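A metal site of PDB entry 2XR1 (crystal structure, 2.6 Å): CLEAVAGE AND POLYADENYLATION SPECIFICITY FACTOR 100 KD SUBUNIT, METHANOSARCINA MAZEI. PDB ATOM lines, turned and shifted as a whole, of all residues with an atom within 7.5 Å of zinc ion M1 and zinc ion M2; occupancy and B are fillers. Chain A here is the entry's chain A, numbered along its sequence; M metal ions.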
ATOM      1  N   VAL A 195     -35.524 -24.744   3.566  1.00  0.00           N
ATOM      2  CA  VAL A 195     -34.430 -24.550   2.639  1.00  0.00           C
ATOM      3  C   VAL A 195     -33.512 -23.573   3.351  1.00  0.00           C
ATOM      4  O   VAL A 195     -33.990 -22.545   3.879  1.00  0.00           O
ATOM      5  CB  VAL A 195     -34.927 -23.903   1.343  1.00  0.00           C
ATOM      6  CG1 VAL A 195     -33.753 -23.420   0.549  1.00  0.00           C
ATOM      7  CG2 VAL A 195     -35.719 -24.892   0.545  1.00  0.00           C
ATOM      8  N   GLY A 196     -32.219 -23.842   3.385  1.00  0.00           N
ATOM      9  CA  GLY A 196     -31.324 -22.917   4.051  1.00  0.00           C
ATOM     10  C   GLY A 196     -30.605 -23.575   5.215  1.00  0.00           C
ATOM     11  O   GLY A 196     -31.120 -24.466   5.878  1.00  0.00           O
ATOM     12  N   SER A 198     -28.244 -25.663   5.628  1.00  0.00           N
ATOM     13  CA  SER A 198     -27.875 -27.075   5.658  1.00  0.00           C
ATOM     14  C   SER A 198     -26.631 -27.227   6.468  1.00  0.00           C
ATOM     15  O   SER A 198     -25.700 -26.442   6.320  1.00  0.00           O
ATOM     16  CB  SER A 198     -27.614 -27.620   4.248  1.00  0.00           C
ATOM     17  OG  SER A 198     -28.857 -27.912   3.587  1.00  0.00           O
ATOM     18  N   ASP A 212     -21.733 -30.071   5.119  1.00  0.00           N
ATOM     19  CA  ASP A 212     -22.243 -28.719   4.841  1.00  0.00           C
ATOM     20  C   ASP A 212     -22.309 -27.804   6.079  1.00  0.00           C
ATOM     21  O   ASP A 212     -22.341 -28.267   7.220  1.00  0.00           O
ATOM     22  CB  ASP A 212     -23.575 -28.759   4.064  1.00  0.00           C
ATOM     23  CG  ASP A 212     -23.402 -29.241   2.572  1.00  0.00           C
ATOM     24  OD1 ASP A 212     -22.250 -29.185   2.059  1.00  0.00           O
ATOM     25  OD2 ASP A 212     -24.417 -29.678   1.915  1.00  0.00           O
ATOM     26  N   VAL A 217     -31.426 -18.898   4.141  1.00  0.00           N
ATOM     27  CA  VAL A 217     -32.102 -18.356   2.976  1.00  0.00           C
ATOM     28  C   VAL A 217     -33.491 -18.074   3.498  1.00  0.00           C
ATOM     29  O   VAL A 217     -34.149 -18.999   3.964  1.00  0.00           O
ATOM     30  CB  VAL A 217     -32.214 -19.424   1.860  1.00  0.00           C
ATOM     31  CG1 VAL A 217     -33.159 -18.942   0.774  1.00  0.00           C
ATOM     32  CG2 VAL A 217     -30.828 -19.794   1.302  1.00  0.00           C
ATOM     33  N   THR A 244     -20.729 -30.166  -0.142  1.00  0.00           N
ATOM     34  CA  THR A 244     -21.334 -30.904  -1.221  1.00  0.00           C
ATOM     35  C   THR A 244     -21.291 -30.106  -2.531  1.00  0.00           C
ATOM     36  O   THR A 244     -21.035 -30.663  -3.604  1.00  0.00           O
ATOM     37  CB  THR A 244     -22.803 -31.235  -0.896  1.00  0.00           C
ATOM     38  OG1 THR A 244     -23.555 -30.025  -0.819  1.00  0.00           O
ATOM     39  CG2 THR A 244     -22.949 -31.948   0.444  1.00  0.00           C
ATOM     40  N   HIS A 245     -21.555 -28.818  -2.442  1.00  0.00           N
ATOM     41  CA  HIS A 245     -21.453 -27.949  -3.602  1.00  0.00           C
ATOM     42  C   HIS A 245     -21.334 -26.499  -3.161  1.00  0.00           C
ATOM     43  O   HIS A 245     -21.416 -26.191  -1.985  1.00  0.00           O
ATOM     44  CB  HIS A 245     -22.625 -28.167  -4.596  1.00  0.00           C
ATOM     45  CG  HIS A 245     -23.969 -27.710  -4.092  1.00  0.00           C
ATOM     46  ND1 HIS A 245     -24.649 -28.374  -3.109  1.00  0.00           N
ATOM     47  CD2 HIS A 245     -24.754 -26.678  -4.468  1.00  0.00           C
ATOM     48  CE1 HIS A 245     -25.792 -27.761  -2.888  1.00  0.00           C
ATOM     49  NE2 HIS A 245     -25.897 -26.732  -3.705  1.00  0.00           N
ATOM     50  N   ALA A 246     -21.108 -25.600  -4.114  1.00  0.00           N
ATOM     51  CA  ALA A 246     -20.586 -24.291  -3.793  1.00  0.00           C
ATOM     52  C   ALA A 246     -21.644 -23.284  -3.347  1.00  0.00           C
ATOM     53  O   ALA A 246     -21.308 -22.173  -2.935  1.00  0.00           O
ATOM     54  CB  ALA A 246     -19.808 -23.765  -4.961  1.00  0.00           C
ATOM     55  N   HIS A 247     -22.913 -23.629  -3.431  1.00  0.00           N
ATOM     56  CA  HIS A 247     -23.959 -22.692  -3.064  1.00  0.00           C
ATOM     57  C   HIS A 247     -23.805 -22.207  -1.628  1.00  0.00           C
ATOM     58  O   HIS A 247     -23.502 -22.991  -0.726  1.00  0.00           O
ATOM     59  CB  HIS A 247     -25.352 -23.321  -3.240  1.00  0.00           C
ATOM     60  CG  HIS A 247     -25.859 -23.290  -4.633  1.00  0.00           C
ATOM     61  ND1 HIS A 247     -26.745 -24.226  -5.118  1.00  0.00           N
ATOM     62  CD2 HIS A 247     -25.624 -22.417  -5.645  1.00  0.00           C
ATOM     63  CE1 HIS A 247     -27.044 -23.933  -6.375  1.00  0.00           C
ATOM     64  NE2 HIS A 247     -26.361 -22.852  -6.719  1.00  0.00           N
ATOM     65  N   LEU A 248     -24.059 -20.913  -1.431  1.00  0.00           N
ATOM     66  CA  LEU A 248     -23.945 -20.285  -0.108  1.00  0.00           C
ATOM     67  C   LEU A 248     -24.745 -20.971   0.985  1.00  0.00           C
ATOM     68  O   LEU A 248     -24.326 -20.984   2.146  1.00  0.00           O
ATOM     69  CB  LEU A 248     -24.319 -18.796  -0.165  1.00  0.00           C
ATOM     70  CG  LEU A 248     -23.080 -17.956  -0.451  1.00  0.00           C
ATOM     71  CD1 LEU A 248     -23.454 -16.571  -0.895  1.00  0.00           C
ATOM     72  CD2 LEU A 248     -22.121 -17.949   0.751  1.00  0.00           C
ATOM     73  N   ASP A 249     -25.879 -21.532   0.621  1.00  0.00           N
ATOM     74  CA  ASP A 249     -26.736 -22.225   1.571  1.00  0.00           C
ATOM     75  C   ASP A 249     -26.154 -23.570   1.907  1.00  0.00           C
ATOM     76  O   ASP A 249     -26.783 -24.313   2.581  1.00  0.00           O
ATOM     77  CB  ASP A 249     -28.202 -22.332   1.079  1.00  0.00           C
ATOM     78  CG  ASP A 249     -28.373 -23.177  -0.233  1.00  0.00           C
ATOM     79  OD1 ASP A 249     -27.734 -22.855  -1.248  1.00  0.00           O
ATOM     80  OD2 ASP A 249     -29.203 -24.135  -0.264  1.00  0.00           O
ATOM     81  N   HIS A 250     -24.935 -23.881   1.474  1.00  0.00           N
ATOM     82  CA  HIS A 250     -24.233 -25.118   1.918  1.00  0.00           C
ATOM     83  C   HIS A 250     -22.823 -24.951   2.405  1.00  0.00           C
ATOM     84  O   HIS A 250     -22.376 -25.831   3.136  1.00  0.00           O
ATOM     85  CB  HIS A 250     -24.219 -26.136   0.795  1.00  0.00           C
ATOM     86  CG  HIS A 250     -25.585 -26.534   0.379  1.00  0.00           C
ATOM     87  ND1 HIS A 250     -26.148 -27.742   0.716  1.00  0.00           N
ATOM     88  CD2 HIS A 250     -26.542 -25.832  -0.289  1.00  0.00           C
ATOM     89  CE1 HIS A 250     -27.387 -27.780   0.245  1.00  0.00           C
ATOM     90  NE2 HIS A 250     -27.646 -26.638  -0.369  1.00  0.00           N
ATOM     91  N   HIS A 332     -26.260 -30.820 -10.347  1.00  0.00           N
ATOM     92  CA  HIS A 332     -26.933 -29.620  -9.820  1.00  0.00           C
ATOM     93  C   HIS A 332     -26.179 -28.371 -10.268  1.00  0.00           C
ATOM     94  O   HIS A 332     -26.725 -27.542 -10.979  1.00  0.00           O
ATOM     95  CB  HIS A 332     -26.995 -29.715  -8.295  1.00  0.00           C
ATOM     96  CG  HIS A 332     -27.556 -28.509  -7.599  1.00  0.00           C
ATOM     97  ND1 HIS A 332     -28.822 -28.028  -7.843  1.00  0.00           N
ATOM     98  CD2 HIS A 332     -27.036 -27.724  -6.626  1.00  0.00           C
ATOM     99  CE1 HIS A 332     -29.045 -26.973  -7.062  1.00  0.00           C
ATOM    100  NE2 HIS A 332     -27.986 -26.787  -6.305  1.00  0.00           N
ATOM    101  N   ILE A 333     -24.936 -28.246  -9.874  1.00  0.00           N
ATOM    102  CA  ILE A 333     -24.059 -27.216 -10.431  1.00  0.00           C
ATOM    103  C   ILE A 333     -22.644 -27.766 -10.584  1.00  0.00           C
ATOM    104  O   ILE A 333     -22.300 -28.847 -10.076  1.00  0.00           O
ATOM    105  CB  ILE A 333     -23.985 -25.935  -9.561  1.00  0.00           C
ATOM    106  CG1 ILE A 333     -23.354 -26.228  -8.186  1.00  0.00           C
ATOM    107  CG2 ILE A 333     -25.350 -25.290  -9.440  1.00  0.00           C
ATOM    108  CD1 ILE A 333     -23.018 -25.013  -7.387  1.00  0.00           C
ATOM    109  N   SER A 336     -20.994 -30.176  -8.235  1.00  0.00           N
ATOM    110  CA  SER A 336     -21.894 -30.641  -7.196  1.00  0.00           C
ATOM    111  C   SER A 336     -21.700 -32.111  -6.980  1.00  0.00           C
ATOM    112  O   SER A 336     -21.519 -32.870  -7.935  1.00  0.00           O
ATOM    113  CB  SER A 336     -23.350 -30.332  -7.497  1.00  0.00           C
ATOM    114  OG  SER A 336     -23.860 -31.035  -8.612  1.00  0.00           O
ATOM    115  N   GLY A 354     -26.986 -34.138  -1.116  1.00  0.00           N
ATOM    116  CA  GLY A 354     -26.893 -32.704  -1.367  1.00  0.00           C
ATOM    117  C   GLY A 354     -27.996 -32.306  -2.333  1.00  0.00           C
ATOM    118  O   GLY A 354     -29.050 -32.972  -2.406  1.00  0.00           O
ATOM    119  N   ASP A 355     -27.790 -31.222  -3.071  1.00  0.00           N
ATOM    120  CA  ASP A 355     -28.762 -30.811  -4.077  1.00  0.00           C
ATOM    121  C   ASP A 355     -28.406 -31.592  -5.338  1.00  0.00           C
ATOM    122  O   ASP A 355     -27.210 -31.791  -5.608  1.00  0.00           O
ATOM    123  CB  ASP A 355     -28.713 -29.296  -4.297  1.00  0.00           C
ATOM    124  CG  ASP A 355     -29.194 -28.469  -3.053  1.00  0.00           C
ATOM    125  OD1 ASP A 355     -29.674 -29.068  -2.032  1.00  0.00           O
ATOM    126  OD2 ASP A 355     -29.066 -27.215  -3.107  1.00  0.00           O
ATOM    127  N   TYR A 356     -29.398 -32.084  -6.065  1.00  0.00           N
ATOM    128  CA  TYR A 356     -29.144 -32.918  -7.252  1.00  0.00           C
ATOM    129  C   TYR A 356     -30.215 -32.913  -8.341  1.00  0.00           C
ATOM    130  O   TYR A 356     -31.337 -32.514  -8.118  1.00  0.00           O
ATOM    131  CB  TYR A 356     -28.934 -34.368  -6.823  1.00  0.00           C
ATOM    132  CG  TYR A 356     -30.159 -35.093  -6.294  1.00  0.00           C
ATOM    133  CD1 TYR A 356     -30.466 -35.069  -4.957  1.00  0.00           C
ATOM    134  CD2 TYR A 356     -30.965 -35.835  -7.133  1.00  0.00           C
ATOM    135  CE1 TYR A 356     -31.566 -35.753  -4.464  1.00  0.00           C
ATOM    136  CE2 TYR A 356     -32.089 -36.513  -6.665  1.00  0.00           C
ATOM    137  CZ  TYR A 356     -32.384 -36.468  -5.332  1.00  0.00           C
ATOM    138  OH  TYR A 356     -33.481 -37.146  -4.851  1.00  0.00           O
ATOM    139  N   GLU A 380     -32.309 -34.408  -0.599  1.00  0.00           N
ATOM    140  CA  GLU A 380     -33.022 -33.124  -0.662  1.00  0.00           C
ATOM    141  C   GLU A 380     -34.447 -33.327  -1.074  1.00  0.00           C
ATOM    142  O   GLU A 380     -34.784 -34.385  -1.635  1.00  0.00           O
ATOM    143  CB  GLU A 380     -32.405 -32.175  -1.669  1.00  0.00           C
ATOM    144  CG  GLU A 380     -32.575 -32.576  -3.130  1.00  0.00           C
ATOM    145  CD  GLU A 380     -32.820 -31.377  -4.050  1.00  0.00           C
ATOM    146  OE1 GLU A 380     -33.770 -30.594  -3.796  1.00  0.00           O
ATOM    147  OE2 GLU A 380     -32.049 -31.213  -5.013  1.00  0.00           O
ATOM    148  N   THR A 382     -36.437 -30.237  -2.377  1.00  0.00           N
ATOM    149  CA  THR A 382     -36.863 -28.872  -2.729  1.00  0.00           C
ATOM    150  C   THR A 382     -38.172 -28.841  -3.491  1.00  0.00           C
ATOM    151  O   THR A 382     -39.059 -28.036  -3.192  1.00  0.00           O
ATOM    152  CB  THR A 382     -35.831 -28.093  -3.557  1.00  0.00           C
ATOM    153  OG1 THR A 382     -34.491 -28.329  -3.082  1.00  0.00           O
ATOM    154  CG2 THR A 382     -36.167 -26.593  -3.521  1.00  0.00           C
ATOM    155  N   VAL A 421     -23.510 -18.733  -9.633  1.00  0.00           N
ATOM    156  CA  VAL A 421     -23.401 -20.033 -10.245  1.00  0.00           C
ATOM    157  C   VAL A 421     -24.648 -20.879 -10.051  1.00  0.00           C
ATOM    158  O   VAL A 421     -25.150 -21.039  -8.946  1.00  0.00           O
ATOM    159  CB  VAL A 421     -22.209 -20.804  -9.702  1.00  0.00           C
ATOM    160  CG1 VAL A 421     -22.303 -20.909  -8.236  1.00  0.00           C
ATOM    161  CG2 VAL A 421     -22.157 -22.155 -10.366  1.00  0.00           C
ATOM    162  N   TYR A 539     -37.065 -21.764  -8.142  1.00  0.00           N
ATOM    163  CA  TYR A 539     -37.868 -21.506  -6.945  1.00  0.00           C
ATOM    164  C   TYR A 539     -37.324 -20.328  -6.133  1.00  0.00           C
ATOM    165  O   TYR A 539     -36.130 -20.004  -6.193  1.00  0.00           O
ATOM    166  CB  TYR A 539     -37.992 -22.746  -6.036  1.00  0.00           C
ATOM    167  CG  TYR A 539     -36.782 -22.972  -5.181  1.00  0.00           C
ATOM    168  CD1 TYR A 539     -35.645 -23.528  -5.726  1.00  0.00           C
ATOM    169  CD2 TYR A 539     -36.776 -22.642  -3.834  1.00  0.00           C
ATOM    170  CE1 TYR A 539     -34.495 -23.735  -4.961  1.00  0.00           C
ATOM    171  CE2 TYR A 539     -35.642 -22.854  -3.042  1.00  0.00           C
ATOM    172  CZ  TYR A 539     -34.494 -23.399  -3.620  1.00  0.00           C
ATOM    173  OH  TYR A 539     -33.345 -23.615  -2.884  1.00  0.00           O
ATOM    174  N   SER A 581     -33.735 -24.283 -12.108  1.00  0.00           N
ATOM    175  CA  SER A 581     -33.358 -24.293 -10.706  1.00  0.00           C
ATOM    176  C   SER A 581     -32.165 -25.177 -10.490  1.00  0.00           C
ATOM    177  O   SER A 581     -31.414 -24.957  -9.535  1.00  0.00           O
ATOM    178  CB  SER A 581     -34.519 -24.794  -9.854  1.00  0.00           C
ATOM    179  OG  SER A 581     -34.839 -26.129 -10.197  1.00  0.00           O
ATOM    180  N   GLY A 582     -31.978 -26.179 -11.356  1.00  0.00           N
ATOM    181  CA  GLY A 582     -30.930 -27.186 -11.173  1.00  0.00           C
ATOM    182  C   GLY A 582     -31.287 -28.282 -10.174  1.00  0.00           C
ATOM    183  O   GLY A 582     -30.433 -29.063  -9.812  1.00  0.00           O
ATOM    184  N   HIS A 583     -32.550 -28.359  -9.740  1.00  0.00           N
ATOM    185  CA  HIS A 583     -33.053 -29.428  -8.876  1.00  0.00           C
ATOM    186  C   HIS A 583     -33.959 -30.413  -9.590  1.00  0.00           C
ATOM    187  O   HIS A 583     -34.719 -30.040 -10.478  1.00  0.00           O
ATOM    188  CB  HIS A 583     -33.894 -28.854  -7.737  1.00  0.00           C
ATOM    189  CG  HIS A 583     -33.119 -28.031  -6.768  1.00  0.00           C
ATOM    190  ND1 HIS A 583     -32.489 -28.577  -5.677  1.00  0.00           N
ATOM    191  CD2 HIS A 583     -32.885 -26.704  -6.710  1.00  0.00           C
ATOM    192  CE1 HIS A 583     -31.876 -27.616  -5.000  1.00  0.00           C
ATOM    193  NE2 HIS A 583     -32.115 -26.474  -5.594  1.00  0.00           N
ATOM    194  N   GLU A 606     -34.830 -33.650   3.564  1.00  0.00           N
ATOM    195  CA  GLU A 606     -34.386 -32.353   4.064  1.00  0.00           C
ATOM    196  C   GLU A 606     -34.344 -31.368   2.902  1.00  0.00           C
ATOM    197  O   GLU A 606     -34.620 -31.741   1.786  1.00  0.00           O
ATOM    198  CB  GLU A 606     -33.022 -32.500   4.724  1.00  0.00           C
ATOM    199  CG  GLU A 606     -31.996 -33.296   3.895  1.00  0.00           C
ATOM    200  CD  GLU A 606     -31.094 -32.453   2.986  1.00  0.00           C
ATOM    201  OE1 GLU A 606     -30.719 -31.297   3.347  1.00  0.00           O
ATOM    202  OE2 GLU A 606     -30.757 -32.979   1.920  1.00  0.00           O
ATOM    203  N   HIS A 607     -34.016 -30.118   3.149  1.00  0.00           N
ATOM    204  CA  HIS A 607     -33.891 -29.130   2.084  1.00  0.00           C
ATOM    205  C   HIS A 607     -35.178 -28.962   1.258  1.00  0.00           C
ATOM    206  O   HIS A 607     -35.243 -29.230   0.058  1.00  0.00           O
ATOM    207  CB  HIS A 607     -32.708 -29.496   1.209  1.00  0.00           C
ATOM    208  CG  HIS A 607     -32.210 -28.384   0.349  1.00  0.00           C
ATOM    209  ND1 HIS A 607     -32.842 -27.998  -0.797  1.00  0.00           N
ATOM    210  CD2 HIS A 607     -31.111 -27.604   0.454  1.00  0.00           C
ATOM    211  CE1 HIS A 607     -32.163 -27.017  -1.376  1.00  0.00           C
ATOM    212  NE2 HIS A 607     -31.099 -26.768  -0.635  1.00  0.00           N
HETATM  213 ZN    ZN M   1     -29.274 -25.969  -1.565  1.00  0.00          ZN
HETATM  214 ZN    ZN M   2     -27.638 -25.745  -4.254  1.00  0.00          ZN
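The side-chain hydroxyl (OG1) of Thr 244 sits at hydrogen-bond distance from a ring nitrogen (ND1) of His 245.
The backbone NH (N) of His 332 is in hydrogen-bond range of the side-chain hydroxyl (OG) of Ser 336, 3.0 Å away.
The backbone carbonyl oxygen of Val 421 sits at hydrogen-bond distance from a ring nitrogen (NE2) of His 247 (3.1 Å).
O of Gly 582 sits at hydrogen-bond distance from ND1 of His 332, at 2.7 Å.
ND1 of His 607 sits at hydrogen-bond distance from OG1 of Thr 382 (2.8 Å).
A ring nitrogen (ND1) of His 250 is in hydrogen-bond range of the side-chain carboxylate (OD2) of Asp 212 (2.9 Å).
Zinc ion M1 is bound by the side-chain carboxylate (OD2) of Asp 355 (2.0 Å), a ring nitrogen (NE2) of His 250 (2.1 Å), a ring nitrogen (NE2) of His 607 (2.2 Å) and the side-chain carboxylate (OD2) of Asp 249 (2.2 Å).
Zinc ion M1 has four donor atoms within binding distance.
Along chain A the residues within 4 Å of zinc ion M1 span positions 249 to 607.
Within 4 Å of zinc ion M2: His 245, His 247, His 250, His 332 and Asp 355.
Zinc ion M2 is bound by a ring nitrogen (ND1) of His 247 (2.0 Å), a ring nitrogen (NE2) of His 245 (2.1 Å), a ring nitrogen (NE2) of His 332 (2.3 Å) and the side-chain carboxylate of Asp 355 (2.3 Å).
Zinc ion M2 has four donor atoms within binding distance.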
